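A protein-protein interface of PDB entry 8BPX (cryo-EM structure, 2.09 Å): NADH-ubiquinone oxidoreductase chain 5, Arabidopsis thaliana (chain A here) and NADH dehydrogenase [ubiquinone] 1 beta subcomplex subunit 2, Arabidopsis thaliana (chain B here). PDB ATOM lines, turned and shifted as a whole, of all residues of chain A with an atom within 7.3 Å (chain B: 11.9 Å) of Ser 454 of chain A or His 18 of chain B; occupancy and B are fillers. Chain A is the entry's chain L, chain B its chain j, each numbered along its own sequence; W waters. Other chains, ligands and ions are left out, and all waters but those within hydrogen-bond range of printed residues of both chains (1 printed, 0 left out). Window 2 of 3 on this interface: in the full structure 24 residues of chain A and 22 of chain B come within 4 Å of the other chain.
Of the 13 printed residues of chain A, 5 touch a printed residue of chain B. Printed residues of chain A that touch a printed residue of chain B: Ser 373, Ser 374, Ile 453, Ser 454 and Cys 456. Among the printed residues, 9 pairs touch across the chains.
Of the printed residues of chain B, Ser 373 of chain A touches Pro 20 (3.6 Å). Ser 374 of chain A touches just one residue of chain B: Pro 20 (3.8 Å). Ile 453 of chain A touches three residues of chain B. Arg 455 of chain A touches none of the printed residues of chain B. Of chain B, only His 18 comes within 4 Å of Cys 456 of chain A. Lys 13 of chain B touches none of the printed residues of chain A. Of the printed residues of chain A, Val 15 of chain B touches Ile 453 and Ser 454. Of the printed residues of chain A, Thr 16 of chain B touches Ile 453 and Ser 454. Of the printed residues of chain A, His 18 of chain B touches Ser 454 and Cys 456. The nearest residue of chain B that does not touch Ser 454 of chain A is Gly 14 of chain B (4.6 Å).
OG of Ser 454 of chain A is in hydrogen-bond range of O of Thr 16 of chain B (2.8 Å). The backbone carbonyl oxygen (O) of Ser 454 of chain A lies within hydrogen-bond range of a ring nitrogen (NE2) of His 18 of chain B (2.8 Å).
Water W1 lies within hydrogen-bond range of O of Ile 453 of chain A, N of His 18 of chain B and O of Cys 456 of chain A.
SD of Met 359 of chain A lies within hydrogen-bond range of SG of Cys 456 of chain A (3.5 Å). The backbone carbonyl oxygen (O) of Val 17 of chain B is in hydrogen-bond range of the backbone NH (N) of Ile 10 of chain B (3.0 Å). OG1 of Thr 11 of chain B is in hydrogen-bond range of OG1 of Thr 16 of chain B, 2.4 Å away. The backbone carbonyl oxygen of Asp 452 of chain A sits at hydrogen-bond distance from the side-chain sulfur of Cys 456 of chain A, 3.0 Å away. O of Ile 453 of chain A lies within hydrogen-bond range of SG of Cys 456 of chain A.
Among the printed residues, merely in contact across the chains: Ser 373 of chain A with Pro 20 of chain B (3.6 Å), Ser 374 of chain A with Pro 20 of chain B (3.8 Å), Ile 453 of chain A with Val 15 of chain B (3.6 Å), Ile 453 of chain A with Thr 16 of chain B (3.96 Å), Ile 453 of chain A with Val 17 of chain B (3.7 Å), Ser 454 of chain A with Val 15 of chain B (3.6 Å) and Cys 456 of chain A with His 18 of chain B (3.7 Å).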
ATOM      1  N   MET A 359      -4.574   2.771  -6.975  1.00  0.00           N
ATOM      2  CA  MET A 359      -4.180   2.808  -8.375  1.00  0.00           C
ATOM      3  C   MET A 359      -2.871   3.563  -8.590  1.00  0.00           C
ATOM      4  O   MET A 359      -2.648   4.119  -9.669  1.00  0.00           O
ATOM      5  CB  MET A 359      -5.296   3.429  -9.211  1.00  0.00           C
ATOM      6  CG  MET A 359      -6.511   2.541  -9.396  1.00  0.00           C
ATOM      7  SD  MET A 359      -6.087   0.828  -9.723  1.00  0.00           S
ATOM      8  CE  MET A 359      -6.006   0.869 -11.511  1.00  0.00           C
ATOM      9  N   SER A 373     -14.710  -5.549  -8.948  1.00  0.00           N
ATOM     10  CA  SER A 373     -14.347  -6.799  -8.288  1.00  0.00           C
ATOM     11  C   SER A 373     -13.041  -6.696  -7.514  1.00  0.00           C
ATOM     12  O   SER A 373     -12.862  -7.405  -6.520  1.00  0.00           O
ATOM     13  CB  SER A 373     -14.260  -7.925  -9.314  1.00  0.00           C
ATOM     14  OG  SER A 373     -15.518  -8.127  -9.926  1.00  0.00           O
ATOM     15  N   SER A 374     -12.116  -5.841  -7.958  1.00  0.00           N
ATOM     16  CA  SER A 374     -10.830  -5.713  -7.284  1.00  0.00           C
ATOM     17  C   SER A 374     -10.931  -4.918  -5.988  1.00  0.00           C
ATOM     18  O   SER A 374     -10.211  -5.213  -5.031  1.00  0.00           O
ATOM     19  CB  SER A 374      -9.806  -5.067  -8.221  1.00  0.00           C
ATOM     20  OG  SER A 374      -9.716  -3.673  -8.002  1.00  0.00           O
ATOM     21  N   PHE A 375     -11.809  -3.916  -5.932  1.00  0.00           N
ATOM     22  CA  PHE A 375     -12.028  -3.113  -4.732  1.00  0.00           C
ATOM     23  C   PHE A 375     -13.508  -3.162  -4.384  1.00  0.00           C
ATOM     24  O   PHE A 375     -14.247  -2.199  -4.626  1.00  0.00           O
ATOM     25  CB  PHE A 375     -11.557  -1.670  -4.912  1.00  0.00           C
ATOM     26  CG  PHE A 375     -10.253  -1.540  -5.632  1.00  0.00           C
ATOM     27  CD1 PHE A 375     -10.149  -0.763  -6.769  1.00  0.00           C
ATOM     28  CD2 PHE A 375      -9.125  -2.192  -5.168  1.00  0.00           C
ATOM     29  CE1 PHE A 375      -8.941  -0.634  -7.426  1.00  0.00           C
ATOM     30  CE2 PHE A 375      -7.925  -2.075  -5.824  1.00  0.00           C
ATOM     31  CZ  PHE A 375      -7.831  -1.294  -6.955  1.00  0.00           C
ATOM     32  N   PHE A 449      -3.616   0.660 -16.906  1.00  0.00           N
ATOM     33  CA  PHE A 449      -2.287   0.127 -17.227  1.00  0.00           C
ATOM     34  C   PHE A 449      -2.142  -1.177 -16.432  1.00  0.00           C
ATOM     35  O   PHE A 449      -2.607  -1.217 -15.304  1.00  0.00           O
ATOM     36  CB  PHE A 449      -1.277   1.225 -16.848  1.00  0.00           C
ATOM     37  CG  PHE A 449      -1.239   2.444 -17.734  1.00  0.00           C
ATOM     38  CD1 PHE A 449      -1.935   3.593 -17.400  1.00  0.00           C
ATOM     39  CD2 PHE A 449      -0.456   2.471 -18.877  1.00  0.00           C
ATOM     40  CE1 PHE A 449      -1.878   4.726 -18.195  1.00  0.00           C
ATOM     41  CE2 PHE A 449      -0.401   3.602 -19.676  1.00  0.00           C
ATOM     42  CZ  PHE A 449      -1.109   4.730 -19.334  1.00  0.00           C
ATOM     43  N   GLY A 450      -1.580  -2.219 -17.012  1.00  0.00           N
ATOM     44  CA  GLY A 450      -1.318  -3.451 -16.275  1.00  0.00           C
ATOM     45  C   GLY A 450      -0.508  -3.247 -15.028  1.00  0.00           C
ATOM     46  O   GLY A 450      -0.858  -3.868 -14.017  1.00  0.00           O
ATOM     47  N   ARG A 451       0.485  -2.355 -15.055  1.00  0.00           N
ATOM     48  CA  ARG A 451       1.356  -2.178 -13.862  1.00  0.00           C
ATOM     49  C   ARG A 451       0.510  -1.636 -12.698  1.00  0.00           C
ATOM     50  O   ARG A 451       0.874  -1.909 -11.540  1.00  0.00           O
ATOM     51  CB  ARG A 451       2.570  -1.293 -14.174  1.00  0.00           C
ATOM     52  CG  ARG A 451       3.533  -1.073 -13.017  1.00  0.00           C
ATOM     53  CD  ARG A 451       4.769  -0.256 -13.345  1.00  0.00           C
ATOM     54  NE  ARG A 451       4.497   1.127 -13.708  1.00  0.00           N
ATOM     55  CZ  ARG A 451       4.311   2.112 -12.836  1.00  0.00           C
ATOM     56  NH1 ARG A 451       4.355   1.865 -11.538  1.00  0.00           N
ATOM     57  NH2 ARG A 451       4.068   3.337 -13.264  1.00  0.00           N
ATOM     58  N   ASP A 452      -0.579  -0.913 -12.992  1.00  0.00           N
ATOM     59  CA  ASP A 452      -1.454  -0.396 -11.911  1.00  0.00           C
ATOM     60  C   ASP A 452      -2.303  -1.537 -11.306  1.00  0.00           C
ATOM     61  O   ASP A 452      -2.289  -1.653 -10.127  1.00  0.00           O
ATOM     62  CB  ASP A 452      -2.241   0.846 -12.374  1.00  0.00           C
ATOM     63  CG  ASP A 452      -1.406   2.081 -12.631  1.00  0.00           C
ATOM     64  OD1 ASP A 452      -0.485   2.349 -11.848  1.00  0.00           O
ATOM     65  OD2 ASP A 452      -1.696   2.763 -13.602  1.00  0.00           O
ATOM     66  N   ILE A 453      -2.859  -2.410 -12.129  1.00  0.00           N
ATOM     67  CA  ILE A 453      -3.771  -3.524 -11.706  1.00  0.00           C
ATOM     68  C   ILE A 453      -3.014  -4.514 -10.845  1.00  0.00           C
ATOM     69  O   ILE A 453      -3.509  -4.873  -9.812  1.00  0.00           O
ATOM     70  CB  ILE A 453      -4.304  -4.131 -13.026  1.00  0.00           C
ATOM     71  CG1 ILE A 453      -5.450  -3.305 -13.605  1.00  0.00           C
ATOM     72  CG2 ILE A 453      -4.695  -5.589 -12.854  1.00  0.00           C
ATOM     73  CD1 ILE A 453      -6.484  -2.928 -12.581  1.00  0.00           C
ATOM     74  N   SER A 454      -1.756  -4.726 -11.159  1.00  0.00           N
ATOM     75  CA  SER A 454      -0.891  -5.737 -10.556  1.00  0.00           C
ATOM     76  C   SER A 454      -0.264  -5.267  -9.243  1.00  0.00           C
ATOM     77  O   SER A 454       0.298  -6.062  -8.593  1.00  0.00           O
ATOM     78  CB  SER A 454       0.088  -6.074 -11.654  1.00  0.00           C
ATOM     79  OG  SER A 454      -0.441  -7.075 -12.489  1.00  0.00           O
ATOM     80  N   ARG A 455      -0.568  -4.061  -8.820  1.00  0.00           N
ATOM     81  CA  ARG A 455      -0.049  -3.478  -7.577  1.00  0.00           C
ATOM     82  C   ARG A 455      -1.227  -2.942  -6.724  1.00  0.00           C
ATOM     83  O   ARG A 455      -0.927  -2.229  -5.786  1.00  0.00           O
ATOM     84  CB  ARG A 455       0.942  -2.391  -7.962  1.00  0.00           C
ATOM     85  CG  ARG A 455       2.205  -2.852  -8.666  1.00  0.00           C
ATOM     86  CD  ARG A 455       3.074  -1.641  -8.928  1.00  0.00           C
ATOM     87  NE  ARG A 455       4.182  -1.540  -7.999  1.00  0.00           N
ATOM     88  CZ  ARG A 455       5.458  -1.737  -8.321  1.00  0.00           C
ATOM     89  NH1 ARG A 455       5.794  -2.023  -9.567  1.00  0.00           N
ATOM     90  NH2 ARG A 455       6.395  -1.630  -7.396  1.00  0.00           N
ATOM     91  N   CYS A 456      -2.487  -3.342  -6.948  1.00  0.00           N
ATOM     92  CA  CYS A 456      -3.645  -2.805  -6.248  1.00  0.00           C
ATOM     93  C   CYS A 456      -3.821  -3.446  -4.872  1.00  0.00           C
ATOM     94  O   CYS A 456      -3.332  -4.545  -4.597  1.00  0.00           O
ATOM     95  CB  CYS A 456      -4.907  -3.016  -7.077  1.00  0.00           C
ATOM     96  SG  CYS A 456      -4.871  -2.268  -8.712  1.00  0.00           S
ATOM     97  N   HIS A 457      -4.555  -2.741  -4.016  1.00  0.00           N
ATOM     98  CA  HIS A 457      -4.856  -3.161  -2.653  1.00  0.00           C
ATOM     99  C   HIS A 457      -6.010  -2.317  -2.136  1.00  0.00           C
ATOM    100  O   HIS A 457      -6.087  -1.124  -2.433  1.00  0.00           O
ATOM    101  CB  HIS A 457      -3.627  -3.003  -1.751  1.00  0.00           C
ATOM    102  CG  HIS A 457      -3.137  -1.592  -1.647  1.00  0.00           C
ATOM    103  ND1 HIS A 457      -2.036  -1.135  -2.337  1.00  0.00           N
ATOM    104  CD2 HIS A 457      -3.594  -0.539  -0.929  1.00  0.00           C
ATOM    105  CE1 HIS A 457      -1.843   0.141  -2.056  1.00  0.00           C
ATOM    106  NE2 HIS A 457      -2.775   0.527  -1.204  1.00  0.00           N
ATOM    107  N   GLY B   9      -3.388 -14.414  -5.879  1.00  0.00           N
ATOM    108  CA  GLY B   9      -3.856 -13.826  -7.120  1.00  0.00           C
ATOM    109  C   GLY B   9      -3.825 -14.751  -8.324  1.00  0.00           C
ATOM    110  O   GLY B   9      -3.200 -15.811  -8.290  1.00  0.00           O
ATOM    111  N   ILE B  10      -4.506 -14.341  -9.393  1.00  0.00           N
ATOM    112  CA  ILE B  10      -4.577 -15.100 -10.635  1.00  0.00           C
ATOM    113  C   ILE B  10      -3.827 -14.338 -11.718  1.00  0.00           C
ATOM    114  O   ILE B  10      -4.067 -13.141 -11.927  1.00  0.00           O
ATOM    115  CB  ILE B  10      -6.036 -15.355 -11.046  1.00  0.00           C
ATOM    116  CG1 ILE B  10      -6.790 -16.041  -9.905  1.00  0.00           C
ATOM    117  CG2 ILE B  10      -6.101 -16.205 -12.306  1.00  0.00           C
ATOM    118  CD1 ILE B  10      -8.060 -15.341  -9.507  1.00  0.00           C
ATOM    119  N   THR B  11      -2.919 -15.024 -12.406  1.00  0.00           N
ATOM    120  CA  THR B  11      -2.039 -14.407 -13.391  1.00  0.00           C
ATOM    121  C   THR B  11      -2.497 -14.800 -14.789  1.00  0.00           C
ATOM    122  O   THR B  11      -2.564 -15.990 -15.113  1.00  0.00           O
ATOM    123  CB  THR B  11      -0.589 -14.828 -13.167  1.00  0.00           C
ATOM    124  OG1 THR B  11      -0.164 -14.407 -11.863  1.00  0.00           O
ATOM    125  CG2 THR B  11       0.314 -14.195 -14.211  1.00  0.00           C
ATOM    126  N   TYR B  12      -2.805 -13.802 -15.612  1.00  0.00           N
ATOM    127  CA  TYR B  12      -3.244 -14.008 -16.989  1.00  0.00           C
ATOM    128  C   TYR B  12      -2.334 -13.209 -17.911  1.00  0.00           C
ATOM    129  O   TYR B  12      -2.406 -11.975 -17.940  1.00  0.00           O
ATOM    130  CB  TYR B  12      -4.700 -13.590 -17.175  1.00  0.00           C
ATOM    131  CG  TYR B  12      -5.340 -14.130 -18.429  1.00  0.00           C
ATOM    132  CD1 TYR B  12      -4.703 -15.087 -19.202  1.00  0.00           C
ATOM    133  CD2 TYR B  12      -6.561 -13.645 -18.865  1.00  0.00           C
ATOM    134  CE1 TYR B  12      -5.284 -15.572 -20.355  1.00  0.00           C
ATOM    135  CE2 TYR B  12      -7.147 -14.117 -20.016  1.00  0.00           C
ATOM    136  CZ  TYR B  12      -6.507 -15.082 -20.758  1.00  0.00           C
ATOM    137  OH  TYR B  12      -7.092 -15.555 -21.908  1.00  0.00           O
ATOM    138  N   LYS B  13      -1.499 -13.921 -18.673  1.00  0.00           N
ATOM    139  CA  LYS B  13      -0.537 -13.365 -19.622  1.00  0.00           C
ATOM    140  C   LYS B  13       0.136 -12.093 -19.115  1.00  0.00           C
ATOM    141  O   LYS B  13      -0.017 -11.017 -19.702  1.00  0.00           O
ATOM    142  CB  LYS B  13      -1.172 -13.132 -21.005  1.00  0.00           C
ATOM    143  CG  LYS B  13      -2.516 -12.437 -21.071  1.00  0.00           C
ATOM    144  CD  LYS B  13      -2.914 -12.223 -22.521  1.00  0.00           C
ATOM    145  CE  LYS B  13      -3.889 -13.270 -23.032  1.00  0.00           C
ATOM    146  NZ  LYS B  13      -5.287 -13.007 -22.605  1.00  0.00           N
ATOM    147  N   GLY B  14       0.888 -12.215 -18.038  1.00  0.00           N
ATOM    148  CA  GLY B  14       1.657 -11.103 -17.495  1.00  0.00           C
ATOM    149  C   GLY B  14       1.017 -10.339 -16.367  1.00  0.00           C
ATOM    150  O   GLY B  14       1.658 -10.076 -15.352  1.00  0.00           O
ATOM    151  N   VAL B  15      -0.244  -9.970 -16.528  1.00  0.00           N
ATOM    152  CA  VAL B  15      -0.933  -9.166 -15.529  1.00  0.00           C
ATOM    153  C   VAL B  15      -1.463 -10.073 -14.426  1.00  0.00           C
ATOM    154  O   VAL B  15      -2.141 -11.072 -14.691  1.00  0.00           O
ATOM    155  CB  VAL B  15      -2.059  -8.348 -16.178  1.00  0.00           C
ATOM    156  CG1 VAL B  15      -2.860  -7.633 -15.125  1.00  0.00           C
ATOM    157  CG2 VAL B  15      -1.468  -7.358 -17.174  1.00  0.00           C
ATOM    158  N   THR B  16      -1.154  -9.724 -13.182  1.00  0.00           N
ATOM    159  CA  THR B  16      -1.584 -10.473 -12.013  1.00  0.00           C
ATOM    160  C   THR B  16      -2.561  -9.628 -11.209  1.00  0.00           C
ATOM    161  O   THR B  16      -2.254  -8.484 -10.856  1.00  0.00           O
ATOM    162  CB  THR B  16      -0.387 -10.868 -11.146  1.00  0.00           C
ATOM    163  OG1 THR B  16       0.225 -12.044 -11.690  1.00  0.00           O
ATOM    164  CG2 THR B  16      -0.823 -11.150  -9.721  1.00  0.00           C
ATOM    165  N   VAL B  17      -3.731 -10.186 -10.921  1.00  0.00           N
ATOM    166  CA  VAL B  17      -4.757  -9.500 -10.146  1.00  0.00           C
ATOM    167  C   VAL B  17      -4.916 -10.231  -8.822  1.00  0.00           C
ATOM    168  O   VAL B  17      -5.133 -11.448  -8.800  1.00  0.00           O
ATOM    169  CB  VAL B  17      -6.092  -9.427 -10.907  1.00  0.00           C
ATOM    170  CG1 VAL B  17      -7.007  -8.390 -10.270  1.00  0.00           C
ATOM    171  CG2 VAL B  17      -5.854  -9.107 -12.366  1.00  0.00           C
ATOM    172  N   HIS B  18      -4.787  -9.493  -7.725  1.00  0.00           N
ATOM    173  CA  HIS B  18      -4.906 -10.055  -6.390  1.00  0.00           C
ATOM    174  C   HIS B  18      -6.362 -10.094  -5.954  1.00  0.00           C
ATOM    175  O   HIS B  18      -7.103  -9.124  -6.130  1.00  0.00           O
ATOM    176  CB  HIS B  18      -4.092  -9.247  -5.378  1.00  0.00           C
ATOM    177  CG  HIS B  18      -2.757  -8.803  -5.885  1.00  0.00           C
ATOM    178  ND1 HIS B  18      -1.633  -9.595  -5.801  1.00  0.00           N
ATOM    179  CD2 HIS B  18      -2.360  -7.646  -6.465  1.00  0.00           C
ATOM    180  CE1 HIS B  18      -0.603  -8.948  -6.315  1.00  0.00           C
ATOM    181  NE2 HIS B  18      -1.018  -7.764  -6.728  1.00  0.00           N
ATOM    182  N   THR B  19      -6.762 -11.222  -5.379  1.00  0.00           N
ATOM    183  CA  THR B  19      -8.106 -11.327  -4.840  1.00  0.00           C
ATOM    184  C   THR B  19      -8.243 -10.412  -3.622  1.00  0.00           C
ATOM    185  O   THR B  19      -7.288 -10.241  -2.857  1.00  0.00           O
ATOM    186  CB  THR B  19      -8.435 -12.779  -4.477  1.00  0.00           C
ATOM    187  OG1 THR B  19      -9.850 -12.987  -4.553  1.00  0.00           O
ATOM    188  CG2 THR B  19      -7.960 -13.128  -3.079  1.00  0.00           C
ATOM    189  N   PRO B  20      -9.389  -9.769  -3.445  1.00  0.00           N
ATOM    190  CA  PRO B  20      -9.559  -8.876  -2.296  1.00  0.00           C
ATOM    191  C   PRO B  20      -9.664  -9.643  -0.986  1.00  0.00           C
ATOM    192  O   PRO B  20      -9.947 -10.841  -0.952  1.00  0.00           O
ATOM    193  CB  PRO B  20     -10.856  -8.127  -2.614  1.00  0.00           C
ATOM    194  CG  PRO B  20     -11.592  -9.010  -3.548  1.00  0.00           C
ATOM    195  CD  PRO B  20     -10.565  -9.778  -4.331  1.00  0.00           C
ATOM    196  N   LYS B  21      -9.409  -8.925   0.105  1.00  0.00           N
ATOM    197  CA  LYS B  21      -9.557  -9.506   1.431  1.00  0.00           C
ATOM    198  C   LYS B  21     -11.001  -9.925   1.660  1.00  0.00           C
ATOM    199  O   LYS B  21     -11.936  -9.244   1.233  1.00  0.00           O
ATOM    200  CB  LYS B  21      -9.125  -8.507   2.503  1.00  0.00           C
ATOM    201  CG  LYS B  21      -7.630  -8.393   2.684  1.00  0.00           C
ATOM    202  CD  LYS B  21      -7.279  -7.290   3.662  1.00  0.00           C
ATOM    203  CE  LYS B  21      -6.200  -7.740   4.635  1.00  0.00           C
ATOM    204  NZ  LYS B  21      -4.837  -7.385   4.157  1.00  0.00           N
ATOM    205  N   THR B  22     -11.179 -11.060   2.340  1.00  0.00           N
ATOM    206  CA  THR B  22     -12.512 -11.637   2.477  1.00  0.00           C
ATOM    207  C   THR B  22     -13.457 -10.703   3.223  1.00  0.00           C
ATOM    208  O   THR B  22     -14.606 -10.516   2.807  1.00  0.00           O
ATOM    209  CB  THR B  22     -12.426 -13.004   3.166  1.00  0.00           C
ATOM    210  OG1 THR B  22     -13.746 -13.523   3.378  1.00  0.00           O
ATOM    211  CG2 THR B  22     -11.682 -12.917   4.492  1.00  0.00           C
ATOM    212  N   HIS B  24     -13.370  -7.538   3.346  1.00  0.00           N
ATOM    213  CA  HIS B  24     -13.716  -6.411   2.490  1.00  0.00           C
ATOM    214  C   HIS B  24     -14.898  -6.754   1.589  1.00  0.00           C
ATOM    215  O   HIS B  24     -15.873  -5.990   1.500  1.00  0.00           O
ATOM    216  CB  HIS B  24     -12.497  -6.003   1.668  1.00  0.00           C
ATOM    217  CG  HIS B  24     -11.596  -5.047   2.379  1.00  0.00           C
ATOM    218  ND1 HIS B  24     -10.499  -4.469   1.783  1.00  0.00           N
ATOM    219  CD2 HIS B  24     -11.632  -4.564   3.642  1.00  0.00           C
ATOM    220  CE1 HIS B  24      -9.897  -3.673   2.646  1.00  0.00           C
ATOM    221  NE2 HIS B  24     -10.565  -3.713   3.784  1.00  0.00           N
ATOM    222  N   THR B  25     -14.835  -7.912   0.930  1.00  0.00           N
ATOM    223  CA  THR B  25     -15.961  -8.374   0.130  1.00  0.00           C
ATOM    224  C   THR B  25     -17.211  -8.505   0.986  1.00  0.00           C
ATOM    225  O   THR B  25     -18.290  -8.049   0.594  1.00  0.00           O
ATOM    226  CB  THR B  25     -15.632  -9.713  -0.536  1.00  0.00           C
ATOM    227  OG1 THR B  25     -14.476  -9.571  -1.368  1.00  0.00           O
ATOM    228  CG2 THR B  25     -16.796 -10.183  -1.378  1.00  0.00           C
HETATM  229  O   HOH W   1      -4.974  -6.193  -7.082  1.00  0.00           O
